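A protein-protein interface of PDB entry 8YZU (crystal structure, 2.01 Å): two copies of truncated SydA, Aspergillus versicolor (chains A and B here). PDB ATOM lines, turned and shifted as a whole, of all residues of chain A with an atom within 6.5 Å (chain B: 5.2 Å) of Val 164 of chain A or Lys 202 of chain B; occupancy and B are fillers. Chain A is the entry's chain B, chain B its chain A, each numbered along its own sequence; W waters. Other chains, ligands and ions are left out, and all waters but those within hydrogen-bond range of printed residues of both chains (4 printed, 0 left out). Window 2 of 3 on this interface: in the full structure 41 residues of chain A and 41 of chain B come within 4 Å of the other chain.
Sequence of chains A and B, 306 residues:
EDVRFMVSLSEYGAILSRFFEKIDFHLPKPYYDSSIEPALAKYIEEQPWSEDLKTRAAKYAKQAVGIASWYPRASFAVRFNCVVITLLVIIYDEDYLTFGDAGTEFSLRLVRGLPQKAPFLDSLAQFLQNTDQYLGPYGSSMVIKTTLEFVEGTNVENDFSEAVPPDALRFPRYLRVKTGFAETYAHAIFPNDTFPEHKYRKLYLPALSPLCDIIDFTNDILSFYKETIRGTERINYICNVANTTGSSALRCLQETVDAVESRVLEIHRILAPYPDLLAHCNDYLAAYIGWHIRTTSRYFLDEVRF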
ATOM      1  N   ASP A 159     -14.574  -2.958  27.936  1.00  0.00           N
ATOM      2  CA  ASP A 159     -14.171  -3.288  26.569  1.00  0.00           C
ATOM      3  C   ASP A 159     -14.587  -2.219  25.573  1.00  0.00           C
ATOM      4  O   ASP A 159     -14.059  -2.190  24.460  1.00  0.00           O
ATOM      5  CB  ASP A 159     -14.775  -4.611  26.093  1.00  0.00           C
ATOM      6  CG  ASP A 159     -14.491  -5.751  27.030  1.00  0.00           C
ATOM      7  OD1 ASP A 159     -13.683  -5.559  27.968  1.00  0.00           O
ATOM      8  OD2 ASP A 159     -15.059  -6.849  26.816  1.00  0.00           O
ATOM      9  N   PHE A 160     -15.550  -1.378  25.917  1.00  0.00           N
ATOM     10  CA  PHE A 160     -15.976  -0.333  25.006  1.00  0.00           C
ATOM     11  C   PHE A 160     -15.250   0.979  25.246  1.00  0.00           C
ATOM     12  O   PHE A 160     -15.567   1.976  24.593  1.00  0.00           O
ATOM     13  CB  PHE A 160     -17.491  -0.185  25.074  1.00  0.00           C
ATOM     14  CG  PHE A 160     -18.185  -1.458  24.723  1.00  0.00           C
ATOM     15  CD1 PHE A 160     -18.305  -1.843  23.392  1.00  0.00           C
ATOM     16  CD2 PHE A 160     -18.616  -2.330  25.715  1.00  0.00           C
ATOM     17  CE1 PHE A 160     -18.886  -3.041  23.063  1.00  0.00           C
ATOM     18  CE2 PHE A 160     -19.207  -3.532  25.386  1.00  0.00           C
ATOM     19  CZ  PHE A 160     -19.334  -3.890  24.065  1.00  0.00           C
ATOM     20  N   SER A 161     -14.225   0.976  26.098  1.00  0.00           N
ATOM     21  CA  SER A 161     -13.428   2.173  26.327  1.00  0.00           C
ATOM     22  C   SER A 161     -12.495   2.394  25.153  1.00  0.00           C
ATOM     23  O   SER A 161     -12.708   1.850  24.065  1.00  0.00           O
ATOM     24  CB  SER A 161     -12.594   2.078  27.601  1.00  0.00           C
ATOM     25  OG  SER A 161     -11.318   1.529  27.317  1.00  0.00           O
ATOM     26  N   GLU A 162     -11.483   3.231  25.353  1.00  0.00           N
ATOM     27  CA  GLU A 162     -10.566   3.587  24.274  1.00  0.00           C
ATOM     28  C   GLU A 162     -11.352   4.037  23.048  1.00  0.00           C
ATOM     29  O   GLU A 162     -10.867   3.955  21.913  1.00  0.00           O
ATOM     30  CB  GLU A 162      -9.622   2.422  23.935  1.00  0.00           C
ATOM     31  CG  GLU A 162      -8.315   2.841  23.258  1.00  0.00           C
ATOM     32  CD  GLU A 162      -7.587   3.932  24.031  1.00  0.00           C
ATOM     33  OE1 GLU A 162      -7.967   5.119  23.894  1.00  0.00           O
ATOM     34  OE2 GLU A 162      -6.629   3.608  24.768  1.00  0.00           O
ATOM     35  N   ALA A 163     -12.588   4.498  23.294  1.00  0.00           N
ATOM     36  CA  ALA A 163     -13.512   4.982  22.267  1.00  0.00           C
ATOM     37  C   ALA A 163     -13.890   3.873  21.292  1.00  0.00           C
ATOM     38  O   ALA A 163     -13.449   3.842  20.139  1.00  0.00           O
ATOM     39  CB  ALA A 163     -12.939   6.169  21.478  1.00  0.00           C
ATOM     40  N   VAL A 164     -14.651   2.917  21.797  1.00  0.00           N
ATOM     41  CA  VAL A 164     -15.180   2.023  20.786  1.00  0.00           C
ATOM     42  C   VAL A 164     -16.652   1.702  20.974  1.00  0.00           C
ATOM     43  O   VAL A 164     -17.124   0.615  20.623  1.00  0.00           O
ATOM     44  CB  VAL A 164     -14.345   0.740  20.725  1.00  0.00           C
ATOM     45  CG1 VAL A 164     -14.704  -0.265  21.748  1.00  0.00           C
ATOM     46  CG2 VAL A 164     -14.434   0.111  19.304  1.00  0.00           C
ATOM     47  N   PRO A 165     -17.467   2.649  21.361  1.00  0.00           N
ATOM     48  CA  PRO A 165     -18.870   2.610  20.886  1.00  0.00           C
ATOM     49  C   PRO A 165     -18.963   3.359  19.577  1.00  0.00           C
ATOM     50  O   PRO A 165     -18.457   4.490  19.455  1.00  0.00           O
ATOM     51  CB  PRO A 165     -19.560   3.317  22.046  1.00  0.00           C
ATOM     52  CG  PRO A 165     -18.452   4.248  22.263  1.00  0.00           C
ATOM     53  CD  PRO A 165     -17.542   3.278  22.683  1.00  0.00           C
ATOM     54  N   PRO A 166     -19.509   2.731  18.601  1.00  0.00           N
ATOM     55  CA  PRO A 166     -19.707   3.382  17.316  1.00  0.00           C
ATOM     56  C   PRO A 166     -20.840   4.371  17.398  1.00  0.00           C
ATOM     57  O   PRO A 166     -21.429   4.537  18.462  1.00  0.00           O
ATOM     58  CB  PRO A 166     -20.042   2.218  16.365  1.00  0.00           C
ATOM     59  CG  PRO A 166     -20.540   1.135  17.274  1.00  0.00           C
ATOM     60  CD  PRO A 166     -19.796   1.288  18.549  1.00  0.00           C
ATOM     61  N   PHE A 171     -27.439   1.276  21.409  1.00  0.00           N
ATOM     62  CA  PHE A 171     -26.478   0.578  22.264  1.00  0.00           C
ATOM     63  C   PHE A 171     -26.395   1.145  23.677  1.00  0.00           C
ATOM     64  O   PHE A 171     -26.374   0.346  24.630  1.00  0.00           O
ATOM     65  CB  PHE A 171     -25.105   0.544  21.582  1.00  0.00           C
ATOM     66  CG  PHE A 171     -24.002  -0.016  22.460  1.00  0.00           C
ATOM     67  CD1 PHE A 171     -24.035  -1.351  22.876  1.00  0.00           C
ATOM     68  CD2 PHE A 171     -22.943   0.789  22.872  1.00  0.00           C
ATOM     69  CE1 PHE A 171     -23.032  -1.867  23.660  1.00  0.00           C
ATOM     70  CE2 PHE A 171     -21.946   0.279  23.686  1.00  0.00           C
ATOM     71  CZ  PHE A 171     -21.989  -1.046  24.072  1.00  0.00           C
ATOM     72  N   ASN A 243     -21.269   9.769  22.764  1.00  0.00           N
ATOM     73  CA  ASN A 243     -20.463   9.250  21.661  1.00  0.00           C
ATOM     74  C   ASN A 243     -21.292   8.707  20.500  1.00  0.00           C
ATOM     75  O   ASN A 243     -20.768   8.621  19.385  1.00  0.00           O
ATOM     76  CB  ASN A 243     -19.519   8.143  22.147  1.00  0.00           C
ATOM     77  CG  ASN A 243     -18.213   8.689  22.714  1.00  0.00           C
ATOM     78  OD1 ASN A 243     -17.669   9.672  22.204  1.00  0.00           O
ATOM     79  ND2 ASN A 243     -17.717   8.064  23.793  1.00  0.00           N
ATOM     80  N   GLU B 197     -15.626 -14.476  21.356  1.00  0.00           N
ATOM     81  CA  GLU B 197     -16.072 -13.276  22.060  1.00  0.00           C
ATOM     82  C   GLU B 197     -14.907 -12.357  22.422  1.00  0.00           C
ATOM     83  O   GLU B 197     -15.026 -11.131  22.312  1.00  0.00           O
ATOM     84  CB  GLU B 197     -16.858 -13.674  23.310  1.00  0.00           C
ATOM     85  CG  GLU B 197     -18.294 -14.110  23.030  1.00  0.00           C
ATOM     86  CD  GLU B 197     -19.119 -14.287  24.303  1.00  0.00           C
ATOM     87  OE1 GLU B 197     -18.610 -13.965  25.398  1.00  0.00           O
ATOM     88  OE2 GLU B 197     -20.277 -14.758  24.213  1.00  0.00           O
ATOM     89  N   LYS B 199     -12.403 -11.399  20.965  1.00  0.00           N
ATOM     90  CA  LYS B 199     -12.070 -10.479  19.883  1.00  0.00           C
ATOM     91  C   LYS B 199     -13.287  -9.784  19.282  1.00  0.00           C
ATOM     92  O   LYS B 199     -13.229  -8.579  19.011  1.00  0.00           O
ATOM     93  CB  LYS B 199     -11.301 -11.220  18.782  1.00  0.00           C
ATOM     94  CG  LYS B 199     -10.682 -10.314  17.714  1.00  0.00           C
ATOM     95  CD  LYS B 199      -9.742 -11.102  16.810  1.00  0.00           C
ATOM     96  CE  LYS B 199      -9.947 -10.774  15.339  1.00  0.00           C
ATOM     97  NZ  LYS B 199      -8.916  -9.830  14.834  1.00  0.00           N
ATOM     98  N   TYR B 200     -14.400 -10.499  19.086  1.00  0.00           N
ATOM     99  CA  TYR B 200     -15.509  -9.977  18.297  1.00  0.00           C
ATOM    100  C   TYR B 200     -16.651  -9.393  19.122  1.00  0.00           C
ATOM    101  O   TYR B 200     -17.444  -8.620  18.574  1.00  0.00           O
ATOM    102  CB  TYR B 200     -16.057 -11.079  17.378  1.00  0.00           C
ATOM    103  CG  TYR B 200     -15.145 -11.353  16.203  1.00  0.00           C
ATOM    104  CD1 TYR B 200     -15.222 -10.580  15.057  1.00  0.00           C
ATOM    105  CD2 TYR B 200     -14.190 -12.362  16.249  1.00  0.00           C
ATOM    106  CE1 TYR B 200     -14.388 -10.803  13.984  1.00  0.00           C
ATOM    107  CE2 TYR B 200     -13.353 -12.599  15.170  1.00  0.00           C
ATOM    108  CZ  TYR B 200     -13.460 -11.807  14.044  1.00  0.00           C
ATOM    109  OH  TYR B 200     -12.638 -12.014  12.961  1.00  0.00           O
ATOM    110  N   ARG B 201     -16.751  -9.728  20.413  1.00  0.00           N
ATOM    111  CA  ARG B 201     -17.892  -9.282  21.207  1.00  0.00           C
ATOM    112  C   ARG B 201     -17.994  -7.764  21.233  1.00  0.00           C
ATOM    113  O   ARG B 201     -19.091  -7.214  21.134  1.00  0.00           O
ATOM    114  CB  ARG B 201     -17.797  -9.830  22.626  1.00  0.00           C
ATOM    115  CG  ARG B 201     -18.972  -9.474  23.515  1.00  0.00           C
ATOM    116  CD  ARG B 201     -18.789 -10.070  24.899  1.00  0.00           C
ATOM    117  NE  ARG B 201     -17.540  -9.626  25.515  1.00  0.00           N
ATOM    118  CZ  ARG B 201     -16.736 -10.405  26.228  1.00  0.00           C
ATOM    119  NH1 ARG B 201     -17.001 -11.693  26.416  1.00  0.00           N
ATOM    120  NH2 ARG B 201     -15.634  -9.883  26.763  1.00  0.00           N
ATOM    121  N   LYS B 202     -16.865  -7.065  21.367  1.00  0.00           N
ATOM    122  CA  LYS B 202     -16.901  -5.603  21.368  1.00  0.00           C
ATOM    123  C   LYS B 202     -17.315  -5.030  20.012  1.00  0.00           C
ATOM    124  O   LYS B 202     -17.773  -3.880  19.941  1.00  0.00           O
ATOM    125  CB  LYS B 202     -15.531  -5.060  21.802  1.00  0.00           C
ATOM    126  CG  LYS B 202     -14.602  -4.692  20.672  1.00  0.00           C
ATOM    127  CD  LYS B 202     -13.148  -4.553  21.122  1.00  0.00           C
ATOM    128  CE  LYS B 202     -12.834  -3.130  21.526  1.00  0.00           C
ATOM    129  NZ  LYS B 202     -11.386  -2.879  21.827  1.00  0.00           N
ATOM    130  N   LEU B 203     -17.171  -5.805  18.938  1.00  0.00           N
ATOM    131  CA  LEU B 203     -17.536  -5.350  17.604  1.00  0.00           C
ATOM    132  C   LEU B 203     -19.017  -5.545  17.294  1.00  0.00           C
ATOM    133  O   LEU B 203     -19.627  -4.668  16.670  1.00  0.00           O
ATOM    134  CB  LEU B 203     -16.687  -6.075  16.559  1.00  0.00           C
ATOM    135  CG  LEU B 203     -15.173  -5.986  16.754  1.00  0.00           C
ATOM    136  CD1 LEU B 203     -14.464  -6.844  15.724  1.00  0.00           C
ATOM    137  CD2 LEU B 203     -14.674  -4.545  16.690  1.00  0.00           C
ATOM    138  N   TYR B 204     -19.626  -6.676  17.692  1.00  0.00           N
ATOM    139  CA  TYR B 204     -21.023  -6.912  17.342  1.00  0.00           C
ATOM    140  C   TYR B 204     -22.005  -6.566  18.452  1.00  0.00           C
ATOM    141  O   TYR B 204     -23.200  -6.464  18.170  1.00  0.00           O
ATOM    142  CB  TYR B 204     -21.260  -8.367  16.891  1.00  0.00           C
ATOM    143  CG  TYR B 204     -20.990  -9.452  17.920  1.00  0.00           C
ATOM    144  CD1 TYR B 204     -21.793  -9.612  19.049  1.00  0.00           C
ATOM    145  CD2 TYR B 204     -19.941 -10.338  17.739  1.00  0.00           C
ATOM    146  CE1 TYR B 204     -21.530 -10.617  19.978  1.00  0.00           C
ATOM    147  CE2 TYR B 204     -19.676 -11.341  18.649  1.00  0.00           C
ATOM    148  CZ  TYR B 204     -20.468 -11.480  19.770  1.00  0.00           C
ATOM    149  OH  TYR B 204     -20.175 -12.488  20.676  1.00  0.00           O
ATOM    150  N   LEU B 205     -21.566  -6.383  19.694  1.00  0.00           N
ATOM    151  CA  LEU B 205     -22.537  -6.040  20.734  1.00  0.00           C
ATOM    152  C   LEU B 205     -23.358  -4.785  20.455  1.00  0.00           C
ATOM    153  O   LEU B 205     -24.550  -4.784  20.810  1.00  0.00           O
ATOM    154  CB  LEU B 205     -21.862  -5.931  22.103  1.00  0.00           C
ATOM    155  CG  LEU B 205     -22.444  -6.928  23.110  1.00  0.00           C
ATOM    156  CD1 LEU B 205     -22.150  -8.359  22.724  1.00  0.00           C
ATOM    157  CD2 LEU B 205     -21.920  -6.645  24.508  1.00  0.00           C
ATOM    158  N   PRO B 206     -22.811  -3.697  19.900  1.00  0.00           N
ATOM    159  CA  PRO B 206     -23.653  -2.516  19.656  1.00  0.00           C
ATOM    160  C   PRO B 206     -24.824  -2.779  18.735  1.00  0.00           C
ATOM    161  O   PRO B 206     -25.809  -2.044  18.817  1.00  0.00           O
ATOM    162  CB  PRO B 206     -22.672  -1.499  19.051  1.00  0.00           C
ATOM    163  CG  PRO B 206     -21.353  -1.860  19.653  1.00  0.00           C
ATOM    164  CD  PRO B 206     -21.380  -3.379  19.704  1.00  0.00           C
HETATM  165  O   HOH W   1     -11.547  -1.004  23.839  1.00  0.00           O
HETATM  166  O   HOH W   2     -17.064  -1.566  18.478  1.00  0.00           O
HETATM  167  O   HOH W   3     -16.864  -6.946  25.070  1.00  0.00           O
HETATM  168  O   HOH W   4     -27.329   0.372  18.807  1.00  0.00           O
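The guanidinium group of Arg 201 of chain B is in salt-bridge range of the side-chain carboxylate of Asp 159 of chain A.
The side-chain carboxylate of Glu 197 of chain B is in salt-bridge range of the guanidinium group of Arg 201 of chain B, 3.0 Å away.
Among the printed residues, pairs that only touch across the chains: Asp 159 of chain A with Lys 202 of chain B, Phe 160 of chain A with Lys 202 of chain B, Val 164 of chain A with Lys 202 of chain B, Phe 171 of chain A with Pro 206 of chain B, Pro 166 of chain A with Pro 206 of chain B and Phe 160 of chain A with Leu 205 of chain B.
Val 164 of chain A touches just one residue of chain B: Lys 202.
Of the printed residues of chain B, Phe 171 of chain A touches Pro 206.
Printed residues of chain A within 4 Å of Arg 201 of chain B: Asp 159.
Of the printed residues of chain A, Leu 205 of chain B touches Phe 160.
Printed residues of chain B within 4 Å of Phe 160 of chain A: Lys 202 (3.4 Å) and Leu 205 (3.8 Å).
Of the printed residues of chain B, Pro 166 of chain A touches Pro 206.
Pro 165 of chain A touches none of the printed residues of chain B.
Tyr 200 of chain B touches none of the printed residues of chain A.
The nearest residue of chain A that does not touch Lys 202 of chain B is Ser 161 of chain A (5.4 Å).
The nearest printed residue of chain B that does not touch Pro 166 of chain A is Lys 202 of chain B (5.7 Å).
Of the 10 printed residues of chain A, 5 touch a printed residue of chain B.
Printed residues of chain A that touch a printed residue of chain B: Asp 159, Phe 160, Val 164, Pro 166 and Phe 171.
Hydrophobic or aromatic side chains of chain A within 4 Å of the printed part of chain B: Phe 160, Val 164, Pro 166 and Phe 171.
Of the 9 printed residues of chain B, 4 touch a printed residue of chain A.
Among the printed residues, Asp or Glu carboxylates within 4 Å of a Lys or Arg side-chain nitrogen of the other chain: Asp 159 of chain A with Arg 201 of chain B (3.1 Å).
No position is printed for both chains.
Water W3 lies within hydrogen-bond range of OD2 of Asp 159 of chain A (2.5 Å) and NE of Arg 201 of chain B (2.8 Å).
Water W1 lies within hydrogen-bond range of NZ of Lys 202 of chain B (2.8 Å), O of Asp 159 of chain A (2.8 Å) and O of Ser 161 of chain A (3.1 Å).
Water W4 bridges N of Phe 171 of chain A and O of Pro 206 of chain B.
Water W2 bridges O of Lys 202 of chain B (2.8 Å) and O of Val 164 of chain A (3.1 Å).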
